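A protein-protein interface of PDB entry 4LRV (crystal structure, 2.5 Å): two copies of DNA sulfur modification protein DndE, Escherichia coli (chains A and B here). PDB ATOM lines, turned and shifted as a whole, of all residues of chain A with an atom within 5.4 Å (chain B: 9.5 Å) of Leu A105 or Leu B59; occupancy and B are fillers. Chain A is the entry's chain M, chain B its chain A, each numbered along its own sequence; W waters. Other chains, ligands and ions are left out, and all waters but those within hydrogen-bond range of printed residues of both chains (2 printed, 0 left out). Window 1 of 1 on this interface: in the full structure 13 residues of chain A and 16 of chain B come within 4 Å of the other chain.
Of the 14 printed residues of chain A, 7 touch a printed residue of chain B. Hydrophobic or aromatic side chains of chain A within 4 Å of the printed part of chain B: Leu A20 and Leu A34. Along chain A the printed residues that touch a printed residue of chain B span positions 20 to 107. Hydrophobic or aromatic side chains of chain B that line the printed part of chain A: Ala B8, Leu B59 and Val B60.
NH1 of Arg A38 is in hydrogen-bond range of O of Ala A104 (2.9 Å). The backbone NH (N) of Thr B58 sits at hydrogen-bond distance from the side-chain carboxylate (OE1) of Glu B14 (2.9 Å). The backbone NH of Met B7 sits at hydrogen-bond distance from the backbone carbonyl oxygen of Leu B61 (3.0 Å). OE2 of Glu B14 lies within hydrogen-bond range of N of Leu B59, 3.3 Å away. O of Leu B9 lies within hydrogen-bond range of N of Gly B57, at 2.8 Å. The backbone NH (N) of Ile A26 lies close to the side-chain hydroxyl (OG1) of Thr A24 (3.3 Å).
The backbone carbonyl oxygen of Leu A105 lies within hydrogen-bond range of the backbone NH of Val B60, at 2.9 Å. O of Leu B55 sits close to OD1 of Asn A107, 3.2 Å away. The backbone carbonyl oxygen of Gly B57 lies close to the side-chain amide oxygen of Asn A107. The side-chain carboxylate (OD1) of Asp B62 is in salt-bridge range of the guanidinium group (NH2) of Arg A38 (2.9 Å). The backbone carbonyl oxygen (O) of Val B60 lies within hydrogen-bond range of the guanidinium group (NH2) of Arg A38, at 2.9 Å. The backbone NH of Asn A107 lies within hydrogen-bond range of the backbone carbonyl oxygen of Thr B58.
Water W2 bridges the side-chain carboxylate of Asp B62 (2.7 Å) and the guanidinium group of Arg A38 (2.8 Å). Water W1 bridges the side-chain carboxylate of Asp B62 (2.9 Å) and the backbone carbonyl oxygen of Leu A34 (3.2 Å).
No position is printed for both chains. Of the 19 pairs that touch across the chains among the printed residues, none has its exchanged pair printed and touching as well.
Among the printed residues, merely in contact across the chains: Leu A20 with Thr B58, Leu A20 with Leu B59, Thr A24 with Glu B14, Thr A24 with Leu B59, Leu A34 with Thr B65, Arg A38 with Arg B6, Arg A38 with Leu B61, Leu A105 with Thr B58, Leu A105 with Leu B59, Arg A106 with Thr B58, Asn A107 with Ala B8, Asn A107 with Asp B56 and Asn A107 with Val B60.
Leu A105 touches three residues of chain B. Leu B59 touches just these residues of chain A: Leu A20, Thr A24 and Leu A105. No residue of chain B comes within 4 Å of Ala A104. Of the printed residues of chain B, Arg A38 touches Arg B6 (3.7 Å), Val B60 (2.9 Å), Leu B61 (3.8 Å) and Asp B62 (2.9 Å). Printed residues of chain B within 4 Å of Leu A34: Thr B65 (3.9 Å). Printed residues of chain A within 4 Å of Asp B62: Arg A38. Printed residues of chain B within 4 Å of Arg A106: Thr B58 (3.5 Å). Of the printed residues of chain A, Leu B61 touches Arg A38. Trp B66 touches none of the printed residues of chain A. The nearest residue of chain A that does not touch Leu B59 is Asn A107 (4.1 Å). The nearest printed residue of chain A that does not touch Ala B8 is Leu A105 (7.3 Å).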
ATOM      1  N   LEU A  20     -13.264 -16.058  19.937  1.00  0.00           N
ATOM      2  CA  LEU A  20     -13.791 -14.711  19.753  1.00  0.00           C
ATOM      3  C   LEU A  20     -13.084 -13.713  20.669  1.00  0.00           C
ATOM      4  O   LEU A  20     -12.820 -12.579  20.280  1.00  0.00           O
ATOM      5  CB  LEU A  20     -15.299 -14.696  20.021  1.00  0.00           C
ATOM      6  CG  LEU A  20     -16.095 -13.887  19.010  1.00  0.00           C
ATOM      7  CD1 LEU A  20     -15.867 -14.475  17.627  1.00  0.00           C
ATOM      8  CD2 LEU A  20     -17.571 -13.899  19.357  1.00  0.00           C
ATOM      9  N   THR A  24     -11.305 -10.224  19.361  1.00  0.00           N
ATOM     10  CA  THR A  24     -11.792  -9.005  19.966  1.00  0.00           C
ATOM     11  C   THR A  24     -11.393  -9.175  21.405  1.00  0.00           C
ATOM     12  O   THR A  24     -10.700 -10.135  21.727  1.00  0.00           O
ATOM     13  CB  THR A  24     -13.319  -8.867  19.830  1.00  0.00           C
ATOM     14  OG1 THR A  24     -13.970  -9.929  20.538  1.00  0.00           O
ATOM     15  CG2 THR A  24     -13.731  -8.908  18.368  1.00  0.00           C
ATOM     16  N   ILE A  26     -13.828  -9.150  23.781  1.00  0.00           N
ATOM     17  CA  ILE A  26     -15.093  -9.443  24.458  1.00  0.00           C
ATOM     18  C   ILE A  26     -15.037 -10.747  25.222  1.00  0.00           C
ATOM     19  O   ILE A  26     -14.460 -11.730  24.740  1.00  0.00           O
ATOM     20  CB  ILE A  26     -16.291  -9.423  23.484  1.00  0.00           C
ATOM     21  CG1 ILE A  26     -17.598  -9.466  24.261  1.00  0.00           C
ATOM     22  CG2 ILE A  26     -16.222 -10.577  22.492  1.00  0.00           C
ATOM     23  CD1 ILE A  26     -18.808  -9.378  23.380  1.00  0.00           C
ATOM     24  N   ALA A  31     -20.264 -12.158  25.224  1.00  0.00           N
ATOM     25  CA  ALA A  31     -20.396 -12.673  23.872  1.00  0.00           C
ATOM     26  C   ALA A  31     -21.615 -13.583  23.745  1.00  0.00           C
ATOM     27  O   ALA A  31     -22.323 -13.532  22.739  1.00  0.00           O
ATOM     28  CB  ALA A  31     -19.129 -13.384  23.442  1.00  0.00           C
ATOM     29  N   LEU A  34     -24.785 -11.573  23.614  1.00  0.00           N
ATOM     30  CA  LEU A  34     -24.869 -11.091  22.246  1.00  0.00           C
ATOM     31  C   LEU A  34     -25.306 -12.170  21.267  1.00  0.00           C
ATOM     32  O   LEU A  34     -26.125 -11.919  20.386  1.00  0.00           O
ATOM     33  CB  LEU A  34     -23.519 -10.517  21.806  1.00  0.00           C
ATOM     34  CG  LEU A  34     -23.085  -9.219  22.475  1.00  0.00           C
ATOM     35  CD1 LEU A  34     -21.851  -8.702  21.783  1.00  0.00           C
ATOM     36  CD2 LEU A  34     -24.183  -8.192  22.425  1.00  0.00           C
ATOM     37  N   ALA A  35     -24.754 -13.370  21.419  1.00  0.00           N
ATOM     38  CA  ALA A  35     -25.028 -14.440  20.474  1.00  0.00           C
ATOM     39  C   ALA A  35     -26.443 -14.958  20.663  1.00  0.00           C
ATOM     40  O   ALA A  35     -27.141 -15.220  19.683  1.00  0.00           O
ATOM     41  CB  ALA A  35     -23.994 -15.568  20.594  1.00  0.00           C
ATOM     42  N   ARG A  38     -28.820 -12.452  18.866  1.00  0.00           N
ATOM     43  CA  ARG A  38     -28.616 -12.558  17.421  1.00  0.00           C
ATOM     44  C   ARG A  38     -29.281 -13.822  16.896  1.00  0.00           C
ATOM     45  O   ARG A  38     -29.905 -13.814  15.843  1.00  0.00           O
ATOM     46  CB  ARG A  38     -27.121 -12.569  17.087  1.00  0.00           C
ATOM     47  CG  ARG A  38     -26.781 -12.793  15.606  1.00  0.00           C
ATOM     48  CD  ARG A  38     -27.438 -11.760  14.692  1.00  0.00           C
ATOM     49  NE  ARG A  38     -27.055 -10.399  15.057  1.00  0.00           N
ATOM     50  CZ  ARG A  38     -25.925  -9.813  14.668  1.00  0.00           C
ATOM     51  NH1 ARG A  38     -25.058 -10.468  13.899  1.00  0.00           N
ATOM     52  NH2 ARG A  38     -25.654  -8.577  15.055  1.00  0.00           N
ATOM     53  N   GLY A 101     -25.874 -18.526  17.524  1.00  0.00           N
ATOM     54  CA  GLY A 101     -25.679 -17.087  17.403  1.00  0.00           C
ATOM     55  C   GLY A 101     -24.235 -16.679  17.163  1.00  0.00           C
ATOM     56  O   GLY A 101     -23.969 -15.619  16.593  1.00  0.00           O
ATOM     57  N   ILE A 102     -23.291 -17.516  17.589  1.00  0.00           N
ATOM     58  CA  ILE A 102     -21.880 -17.218  17.377  1.00  0.00           C
ATOM     59  C   ILE A 102     -21.572 -17.210  15.895  1.00  0.00           C
ATOM     60  O   ILE A 102     -20.948 -16.274  15.401  1.00  0.00           O
ATOM     61  CB  ILE A 102     -20.945 -18.168  18.140  1.00  0.00           C
ATOM     62  CG1 ILE A 102     -20.892 -17.762  19.614  1.00  0.00           C
ATOM     63  CG2 ILE A 102     -19.529 -18.129  17.541  1.00  0.00           C
ATOM     64  CD1 ILE A 102     -20.335 -18.824  20.517  1.00  0.00           C
ATOM     65  N   ALA A 103     -22.033 -18.223  15.172  1.00  0.00           N
ATOM     66  CA  ALA A 103     -21.856 -18.215  13.724  1.00  0.00           C
ATOM     67  C   ALA A 103     -22.647 -17.073  13.084  1.00  0.00           C
ATOM     68  O   ALA A 103     -22.277 -16.577  12.025  1.00  0.00           O
ATOM     69  CB  ALA A 103     -22.249 -19.549  13.115  1.00  0.00           C
ATOM     70  N   ALA A 104     -23.723 -16.647  13.742  1.00  0.00           N
ATOM     71  CA  ALA A 104     -24.576 -15.592  13.204  1.00  0.00           C
ATOM     72  C   ALA A 104     -24.077 -14.185  13.550  1.00  0.00           C
ATOM     73  O   ALA A 104     -24.563 -13.200  12.991  1.00  0.00           O
ATOM     74  CB  ALA A 104     -25.982 -15.788  13.662  1.00  0.00           C
ATOM     75  N   LEU A 105     -23.114 -14.102  14.473  1.00  0.00           N
ATOM     76  CA  LEU A 105     -22.399 -12.861  14.755  1.00  0.00           C
ATOM     77  C   LEU A 105     -21.138 -12.705  13.894  1.00  0.00           C
ATOM     78  O   LEU A 105     -20.524 -11.634  13.859  1.00  0.00           O
ATOM     79  CB  LEU A 105     -21.999 -12.798  16.230  1.00  0.00           C
ATOM     80  CG  LEU A 105     -23.008 -12.500  17.336  1.00  0.00           C
ATOM     81  CD1 LEU A 105     -22.294 -12.556  18.703  1.00  0.00           C
ATOM     82  CD2 LEU A 105     -23.643 -11.159  17.159  1.00  0.00           C
ATOM     83  N   ARG A 106     -20.745 -13.779  13.214  1.00  0.00           N
ATOM     84  CA  ARG A 106     -19.467 -13.825  12.512  1.00  0.00           C
ATOM     85  C   ARG A 106     -19.566 -13.015  11.214  1.00  0.00           C
ATOM     86  O   ARG A 106     -20.519 -13.182  10.437  1.00  0.00           O
ATOM     87  CB  ARG A 106     -19.076 -15.290  12.252  1.00  0.00           C
ATOM     88  CG  ARG A 106     -17.619 -15.671  12.581  1.00  0.00           C
ATOM     89  CD  ARG A 106     -17.360 -15.960  14.079  1.00  0.00           C
ATOM     90  NE  ARG A 106     -17.314 -17.397  14.405  1.00  0.00           N
ATOM     91  CZ  ARG A 106     -16.618 -17.943  15.411  1.00  0.00           C
ATOM     92  NH1 ARG A 106     -15.864 -17.204  16.220  1.00  0.00           N
ATOM     93  NH2 ARG A 106     -16.662 -19.255  15.611  1.00  0.00           N
ATOM     94  N   ASN A 107     -18.613 -12.103  11.011  1.00  0.00           N
ATOM     95  CA  ASN A 107     -18.522 -11.326   9.773  1.00  0.00           C
ATOM     96  C   ASN A 107     -17.980 -12.188   8.646  1.00  0.00           C
ATOM     97  O   ASN A 107     -16.881 -12.728   8.751  1.00  0.00           O
ATOM     98  CB  ASN A 107     -17.658 -10.062   9.959  1.00  0.00           C
ATOM     99  CG  ASN A 107     -17.544  -9.199   8.675  1.00  0.00           C
ATOM    100  OD1 ASN A 107     -16.562  -8.468   8.489  1.00  0.00           O
ATOM    101  ND2 ASN A 107     -18.539  -9.282   7.800  1.00  0.00           N
ATOM    102  N   ARG B   6     -26.849  -3.162  11.533  1.00  0.00           N
ATOM    103  CA  ARG B   6     -25.628  -3.776  12.042  1.00  0.00           C
ATOM    104  C   ARG B   6     -24.411  -3.518  11.150  1.00  0.00           C
ATOM    105  O   ARG B   6     -24.539  -3.308   9.944  1.00  0.00           O
ATOM    106  CB  ARG B   6     -25.818  -5.276  12.312  1.00  0.00           C
ATOM    107  CG  ARG B   6     -26.385  -6.057  11.168  1.00  0.00           C
ATOM    108  CD  ARG B   6     -26.388  -7.525  11.486  1.00  0.00           C
ATOM    109  NE  ARG B   6     -27.694  -8.033  11.901  1.00  0.00           N
ATOM    110  CZ  ARG B   6     -28.104  -9.281  11.662  1.00  0.00           C
ATOM    111  NH1 ARG B   6     -27.313 -10.128  11.016  1.00  0.00           N
ATOM    112  NH2 ARG B   6     -29.311  -9.678  12.048  1.00  0.00           N
ATOM    113  N   MET B   7     -23.230  -3.515  11.761  1.00  0.00           N
ATOM    114  CA  MET B   7     -22.010  -3.220  11.021  1.00  0.00           C
ATOM    115  C   MET B   7     -20.798  -3.841  11.661  1.00  0.00           C
ATOM    116  O   MET B   7     -20.856  -4.285  12.809  1.00  0.00           O
ATOM    117  CB  MET B   7     -21.792  -1.708  10.906  1.00  0.00           C
ATOM    118  CG  MET B   7     -21.730  -0.990  12.217  1.00  0.00           C
ATOM    119  SD  MET B   7     -23.284   0.156  12.507  1.00  0.00           S
ATOM    120  CE  MET B   7     -24.518  -1.173  13.093  1.00  0.00           C
ATOM    121  N   ALA B   8     -19.703  -3.856  10.906  1.00  0.00           N
ATOM    122  CA  ALA B   8     -18.421  -4.362  11.374  1.00  0.00           C
ATOM    123  C   ALA B   8     -17.332  -3.289  11.256  1.00  0.00           C
ATOM    124  O   ALA B   8     -17.437  -2.380  10.437  1.00  0.00           O
ATOM    125  CB  ALA B   8     -18.027  -5.609  10.586  1.00  0.00           C
ATOM    126  N   LEU B   9     -16.302  -3.396  12.093  1.00  0.00           N
ATOM    127  CA  LEU B   9     -15.098  -2.586  11.953  1.00  0.00           C
ATOM    128  C   LEU B   9     -14.052  -3.344  11.131  1.00  0.00           C
ATOM    129  O   LEU B   9     -14.307  -4.444  10.653  1.00  0.00           O
ATOM    130  CB  LEU B   9     -14.540  -2.226  13.333  1.00  0.00           C
ATOM    131  CG  LEU B   9     -15.421  -1.226  14.080  1.00  0.00           C
ATOM    132  CD1 LEU B   9     -14.950  -1.018  15.498  1.00  0.00           C
ATOM    133  CD2 LEU B   9     -15.459   0.098  13.338  1.00  0.00           C
ATOM    134  N   SER B  10     -12.876  -2.761  10.951  1.00  0.00           N
ATOM    135  CA  SER B  10     -11.812  -3.495  10.276  1.00  0.00           C
ATOM    136  C   SER B  10     -11.109  -4.385  11.282  1.00  0.00           C
ATOM    137  O   SER B  10     -11.282  -4.231  12.502  1.00  0.00           O
ATOM    138  CB  SER B  10     -10.826  -2.559   9.583  1.00  0.00           C
ATOM    139  OG  SER B  10     -10.176  -1.708  10.504  1.00  0.00           O
ATOM    140  N   ARG B  11     -10.333  -5.331  10.767  1.00  0.00           N
ATOM    141  CA  ARG B  11      -9.539  -6.199  11.606  1.00  0.00           C
ATOM    142  C   ARG B  11      -8.521  -5.350  12.362  1.00  0.00           C
ATOM    143  O   ARG B  11      -8.408  -5.449  13.594  1.00  0.00           O
ATOM    144  CB  ARG B  11      -8.856  -7.275  10.756  1.00  0.00           C
ATOM    145  CG  ARG B  11      -7.886  -8.165  11.513  1.00  0.00           C
ATOM    146  CD  ARG B  11      -8.603  -9.144  12.422  1.00  0.00           C
ATOM    147  NE  ARG B  11      -7.647 -10.018  13.085  1.00  0.00           N
ATOM    148  CZ  ARG B  11      -7.389 -10.021  14.390  1.00  0.00           C
ATOM    149  NH1 ARG B  11      -8.040  -9.198  15.215  1.00  0.00           N
ATOM    150  NH2 ARG B  11      -6.477 -10.867  14.877  1.00  0.00           N
ATOM    151  N   GLU B  14     -10.316  -3.623  15.255  1.00  0.00           N
ATOM    152  CA  GLU B  14     -10.770  -4.538  16.301  1.00  0.00           C
ATOM    153  C   GLU B  14      -9.612  -4.903  17.216  1.00  0.00           C
ATOM    154  O   GLU B  14      -9.743  -4.875  18.442  1.00  0.00           O
ATOM    155  CB  GLU B  14     -11.390  -5.809  15.717  1.00  0.00           C
ATOM    156  CG  GLU B  14     -12.917  -5.793  15.677  1.00  0.00           C
ATOM    157  CD  GLU B  14     -13.534  -7.170  15.375  1.00  0.00           C
ATOM    158  OE1 GLU B  14     -12.775  -8.118  15.051  1.00  0.00           O
ATOM    159  OE2 GLU B  14     -14.784  -7.299  15.479  1.00  0.00           O
ATOM    160  N   LEU B  17      -8.785  -2.152  19.539  1.00  0.00           N
ATOM    161  CA  LEU B  17      -9.810  -2.094  20.582  1.00  0.00           C
ATOM    162  C   LEU B  17      -9.545  -3.132  21.671  1.00  0.00           C
ATOM    163  O   LEU B  17      -9.672  -2.830  22.859  1.00  0.00           O
ATOM    164  CB  LEU B  17     -11.216  -2.257  19.997  1.00  0.00           C
ATOM    165  CG  LEU B  17     -11.648  -1.150  19.029  1.00  0.00           C
ATOM    166  CD1 LEU B  17     -12.906  -1.557  18.281  1.00  0.00           C
ATOM    167  CD2 LEU B  17     -11.872   0.158  19.759  1.00  0.00           C
ATOM    168  N   PRO B  28     -14.633  -3.197  24.098  1.00  0.00           N
ATOM    169  CA  PRO B  28     -14.458  -2.746  22.706  1.00  0.00           C
ATOM    170  C   PRO B  28     -15.573  -1.822  22.205  1.00  0.00           C
ATOM    171  O   PRO B  28     -15.290  -0.807  21.570  1.00  0.00           O
ATOM    172  CB  PRO B  28     -14.436  -4.050  21.908  1.00  0.00           C
ATOM    173  CG  PRO B  28     -14.062  -5.109  22.891  1.00  0.00           C
ATOM    174  CD  PRO B  28     -14.647  -4.670  24.206  1.00  0.00           C
ATOM    175  N   ASN B  29     -16.826  -2.135  22.502  1.00  0.00           N
ATOM    176  CA  ASN B  29     -17.913  -1.288  22.017  1.00  0.00           C
ATOM    177  C   ASN B  29     -17.948   0.125  22.631  1.00  0.00           C
ATOM    178  O   ASN B  29     -18.303   1.089  21.949  1.00  0.00           O
ATOM    179  CB  ASN B  29     -19.274  -1.996  22.109  1.00  0.00           C
ATOM    180  CG  ASN B  29     -19.746  -2.200  23.535  1.00  0.00           C
ATOM    181  OD1 ASN B  29     -18.948  -2.287  24.471  1.00  0.00           O
ATOM    182  ND2 ASN B  29     -21.065  -2.286  23.706  1.00  0.00           N
ATOM    183  N   LEU B  55     -13.466  -3.633   5.593  1.00  0.00           N
ATOM    184  CA  LEU B  55     -14.016  -3.821   6.934  1.00  0.00           C
ATOM    185  C   LEU B  55     -14.149  -5.307   7.263  1.00  0.00           C
ATOM    186  O   LEU B  55     -15.244  -5.879   7.236  1.00  0.00           O
ATOM    187  CB  LEU B  55     -15.331  -3.047   7.139  1.00  0.00           C
ATOM    188  CG  LEU B  55     -15.241  -1.518   6.977  1.00  0.00           C
ATOM    189  CD1 LEU B  55     -16.578  -0.823   7.203  1.00  0.00           C
ATOM    190  CD2 LEU B  55     -14.203  -0.938   7.906  1.00  0.00           C
ATOM    191  N   ASP B  56     -13.005  -5.904   7.594  1.00  0.00           N
ATOM    192  CA  ASP B  56     -12.871  -7.354   7.757  1.00  0.00           C
ATOM    193  C   ASP B  56     -12.766  -7.775   9.223  1.00  0.00           C
ATOM    194  O   ASP B  56     -12.098  -8.755   9.565  1.00  0.00           O
ATOM    195  CB  ASP B  56     -11.670  -7.881   6.950  1.00  0.00           C
ATOM    196  CG  ASP B  56     -10.352  -7.163   7.292  1.00  0.00           C
ATOM    197  OD1 ASP B  56     -10.372  -6.105   7.979  1.00  0.00           O
ATOM    198  OD2 ASP B  56      -9.285  -7.673   6.856  1.00  0.00           O
ATOM    199  N   GLY B  57     -13.439  -7.030  10.088  1.00  0.00           N
ATOM    200  CA  GLY B  57     -13.532  -7.405  11.490  1.00  0.00           C
ATOM    201  C   GLY B  57     -14.259  -8.722  11.650  1.00  0.00           C
ATOM    202  O   GLY B  57     -15.022  -9.146  10.785  1.00  0.00           O
ATOM    203  N   THR B  58     -14.001  -9.364  12.775  1.00  0.00           N
ATOM    204  CA  THR B  58     -14.576 -10.648  13.111  1.00  0.00           C
ATOM    205  C   THR B  58     -16.095 -10.595  13.284  1.00  0.00           C
ATOM    206  O   THR B  58     -16.800 -11.513  12.872  1.00  0.00           O
ATOM    207  CB  THR B  58     -13.935 -11.151  14.410  1.00  0.00           C
ATOM    208  OG1 THR B  58     -12.513 -11.103  14.269  1.00  0.00           O
ATOM    209  CG2 THR B  58     -14.366 -12.567  14.730  1.00  0.00           C
ATOM    210  N   LEU B  59     -16.593  -9.519  13.889  1.00  0.00           N
ATOM    211  CA  LEU B  59     -17.976  -9.473  14.364  1.00  0.00           C
ATOM    212  C   LEU B  59     -18.838  -8.442  13.662  1.00  0.00           C
ATOM    213  O   LEU B  59     -18.440  -7.288  13.548  1.00  0.00           O
ATOM    214  CB  LEU B  59     -17.992  -9.188  15.872  1.00  0.00           C
ATOM    215  CG  LEU B  59     -18.049 -10.378  16.831  1.00  0.00           C
ATOM    216  CD1 LEU B  59     -17.304 -11.594  16.278  1.00  0.00           C
ATOM    217  CD2 LEU B  59     -17.519  -9.987  18.216  1.00  0.00           C
ATOM    218  N   VAL B  60     -20.023  -8.852  13.211  1.00  0.00           N
ATOM    219  CA  VAL B  60     -21.033  -7.891  12.754  1.00  0.00           C
ATOM    220  C   VAL B  60     -22.022  -7.663  13.907  1.00  0.00           C
ATOM    221  O   VAL B  60     -22.939  -8.462  14.120  1.00  0.00           O
ATOM    222  CB  VAL B  60     -21.806  -8.389  11.502  1.00  0.00           C
ATOM    223  CG1 VAL B  60     -22.754  -7.316  11.008  1.00  0.00           C
ATOM    224  CG2 VAL B  60     -20.865  -8.802  10.386  1.00  0.00           C
ATOM    225  N   LEU B  61     -21.817  -6.593  14.668  1.00  0.00           N
ATOM    226  CA  LEU B  61     -22.668  -6.314  15.826  1.00  0.00           C
ATOM    227  C   LEU B  61     -23.775  -5.343  15.488  1.00  0.00           C
ATOM    228  O   LEU B  61     -23.626  -4.516  14.602  1.00  0.00           O
ATOM    229  CB  LEU B  61     -21.846  -5.751  16.984  1.00  0.00           C
ATOM    230  CG  LEU B  61     -20.607  -6.549  17.372  1.00  0.00           C
ATOM    231  CD1 LEU B  61     -19.775  -5.751  18.340  1.00  0.00           C
ATOM    232  CD2 LEU B  61     -20.968  -7.927  17.940  1.00  0.00           C
ATOM    233  N   ASP B  62     -24.887  -5.446  16.203  1.00  0.00           N
ATOM    234  CA  ASP B  62     -25.971  -4.475  16.098  1.00  0.00           C
ATOM    235  C   ASP B  62     -25.503  -3.056  16.359  1.00  0.00           C
ATOM    236  O   ASP B  62     -24.661  -2.809  17.230  1.00  0.00           O
ATOM    237  CB  ASP B  62     -27.084  -4.800  17.096  1.00  0.00           C
ATOM    238  CG  ASP B  62     -27.649  -6.182  16.910  1.00  0.00           C
ATOM    239  OD1 ASP B  62     -27.683  -6.677  15.766  1.00  0.00           O
ATOM    240  OD2 ASP B  62     -28.067  -6.776  17.926  1.00  0.00           O
ATOM    241  N   LYS B  63     -26.067  -2.120  15.612  1.00  0.00           N
ATOM    242  CA  LYS B  63     -25.824  -0.701  15.832  1.00  0.00           C
ATOM    243  C   LYS B  63     -25.981  -0.289  17.294  1.00  0.00           C
ATOM    244  O   LYS B  63     -25.211   0.528  17.792  1.00  0.00           O
ATOM    245  CB  LYS B  63     -26.748   0.138  14.954  1.00  0.00           C
ATOM    246  CG  LYS B  63     -26.403   1.626  14.959  1.00  0.00           C
ATOM    247  CD  LYS B  63     -27.065   2.360  13.801  1.00  0.00           C
ATOM    248  CE  LYS B  63     -28.589   2.308  13.887  1.00  0.00           C
ATOM    249  NZ  LYS B  63     -29.183   2.387  12.535  1.00  0.00           N
ATOM    250  N   THR B  65     -25.634  -2.164  19.966  1.00  0.00           N
ATOM    251  CA  THR B  65     -24.497  -2.711  20.674  1.00  0.00           C
ATOM    252  C   THR B  65     -23.291  -1.783  20.545  1.00  0.00           C
ATOM    253  O   THR B  65     -22.649  -1.462  21.544  1.00  0.00           O
ATOM    254  CB  THR B  65     -24.115  -4.106  20.149  1.00  0.00           C
ATOM    255  OG1 THR B  65     -25.282  -4.930  20.079  1.00  0.00           O
ATOM    256  CG2 THR B  65     -23.113  -4.749  21.068  1.00  0.00           C
ATOM    257  N   TRP B  66     -22.987  -1.367  19.317  1.00  0.00           N
ATOM    258  CA  TRP B  66     -21.856  -0.482  19.085  1.00  0.00           C
ATOM    259  C   TRP B  66     -22.068   0.877  19.736  1.00  0.00           C
ATOM    260  O   TRP B  66     -21.186   1.370  20.448  1.00  0.00           O
ATOM    261  CB  TRP B  66     -21.604  -0.259  17.593  1.00  0.00           C
ATOM    262  CG  TRP B  66     -20.919  -1.381  16.855  1.00  0.00           C
ATOM    263  CD1 TRP B  66     -21.444  -2.115  15.836  1.00  0.00           C
ATOM    264  CD2 TRP B  66     -19.581  -1.862  17.046  1.00  0.00           C
ATOM    265  NE1 TRP B  66     -20.532  -3.032  15.392  1.00  0.00           N
ATOM    266  CE2 TRP B  66     -19.376  -2.898  16.113  1.00  0.00           C
ATOM    267  CE3 TRP B  66     -18.536  -1.522  17.920  1.00  0.00           C
ATOM    268  CZ2 TRP B  66     -18.169  -3.600  16.021  1.00  0.00           C
ATOM    269  CZ3 TRP B  66     -17.335  -2.220  17.824  1.00  0.00           C
ATOM    270  CH2 TRP B  66     -17.168  -3.252  16.884  1.00  0.00           C
ATOM    271  N   TRP B  94     -17.989   6.057   9.542  1.00  0.00           N
ATOM    272  CA  TRP B  94     -18.040   5.714  10.979  1.00  0.00           C
ATOM    273  C   TRP B  94     -16.824   4.872  11.379  1.00  0.00           C
ATOM    274  O   TRP B  94     -16.173   5.159  12.373  1.00  0.00           O
ATOM    275  CB  TRP B  94     -19.358   4.996  11.375  1.00  0.00           C
ATOM    276  CG  TRP B  94     -19.291   4.344  12.762  1.00  0.00           C
ATOM    277  CD1 TRP B  94     -19.325   4.981  13.959  1.00  0.00           C
ATOM    278  CD2 TRP B  94     -19.137   2.940  13.063  1.00  0.00           C
ATOM    279  NE1 TRP B  94     -19.209   4.073  14.988  1.00  0.00           N
ATOM    280  CE2 TRP B  94     -19.092   2.816  14.465  1.00  0.00           C
ATOM    281  CE3 TRP B  94     -19.039   1.781  12.279  1.00  0.00           C
ATOM    282  CZ2 TRP B  94     -18.951   1.581  15.109  1.00  0.00           C
ATOM    283  CZ3 TRP B  94     -18.891   0.560  12.913  1.00  0.00           C
ATOM    284  CH2 TRP B  94     -18.853   0.466  14.321  1.00  0.00           C
HETATM  285  O   HOH W   1     -26.964  -8.990  19.490  1.00  0.00           O
HETATM  286  O   HOH W   2     -28.670  -9.238  17.050  1.00  0.00           O
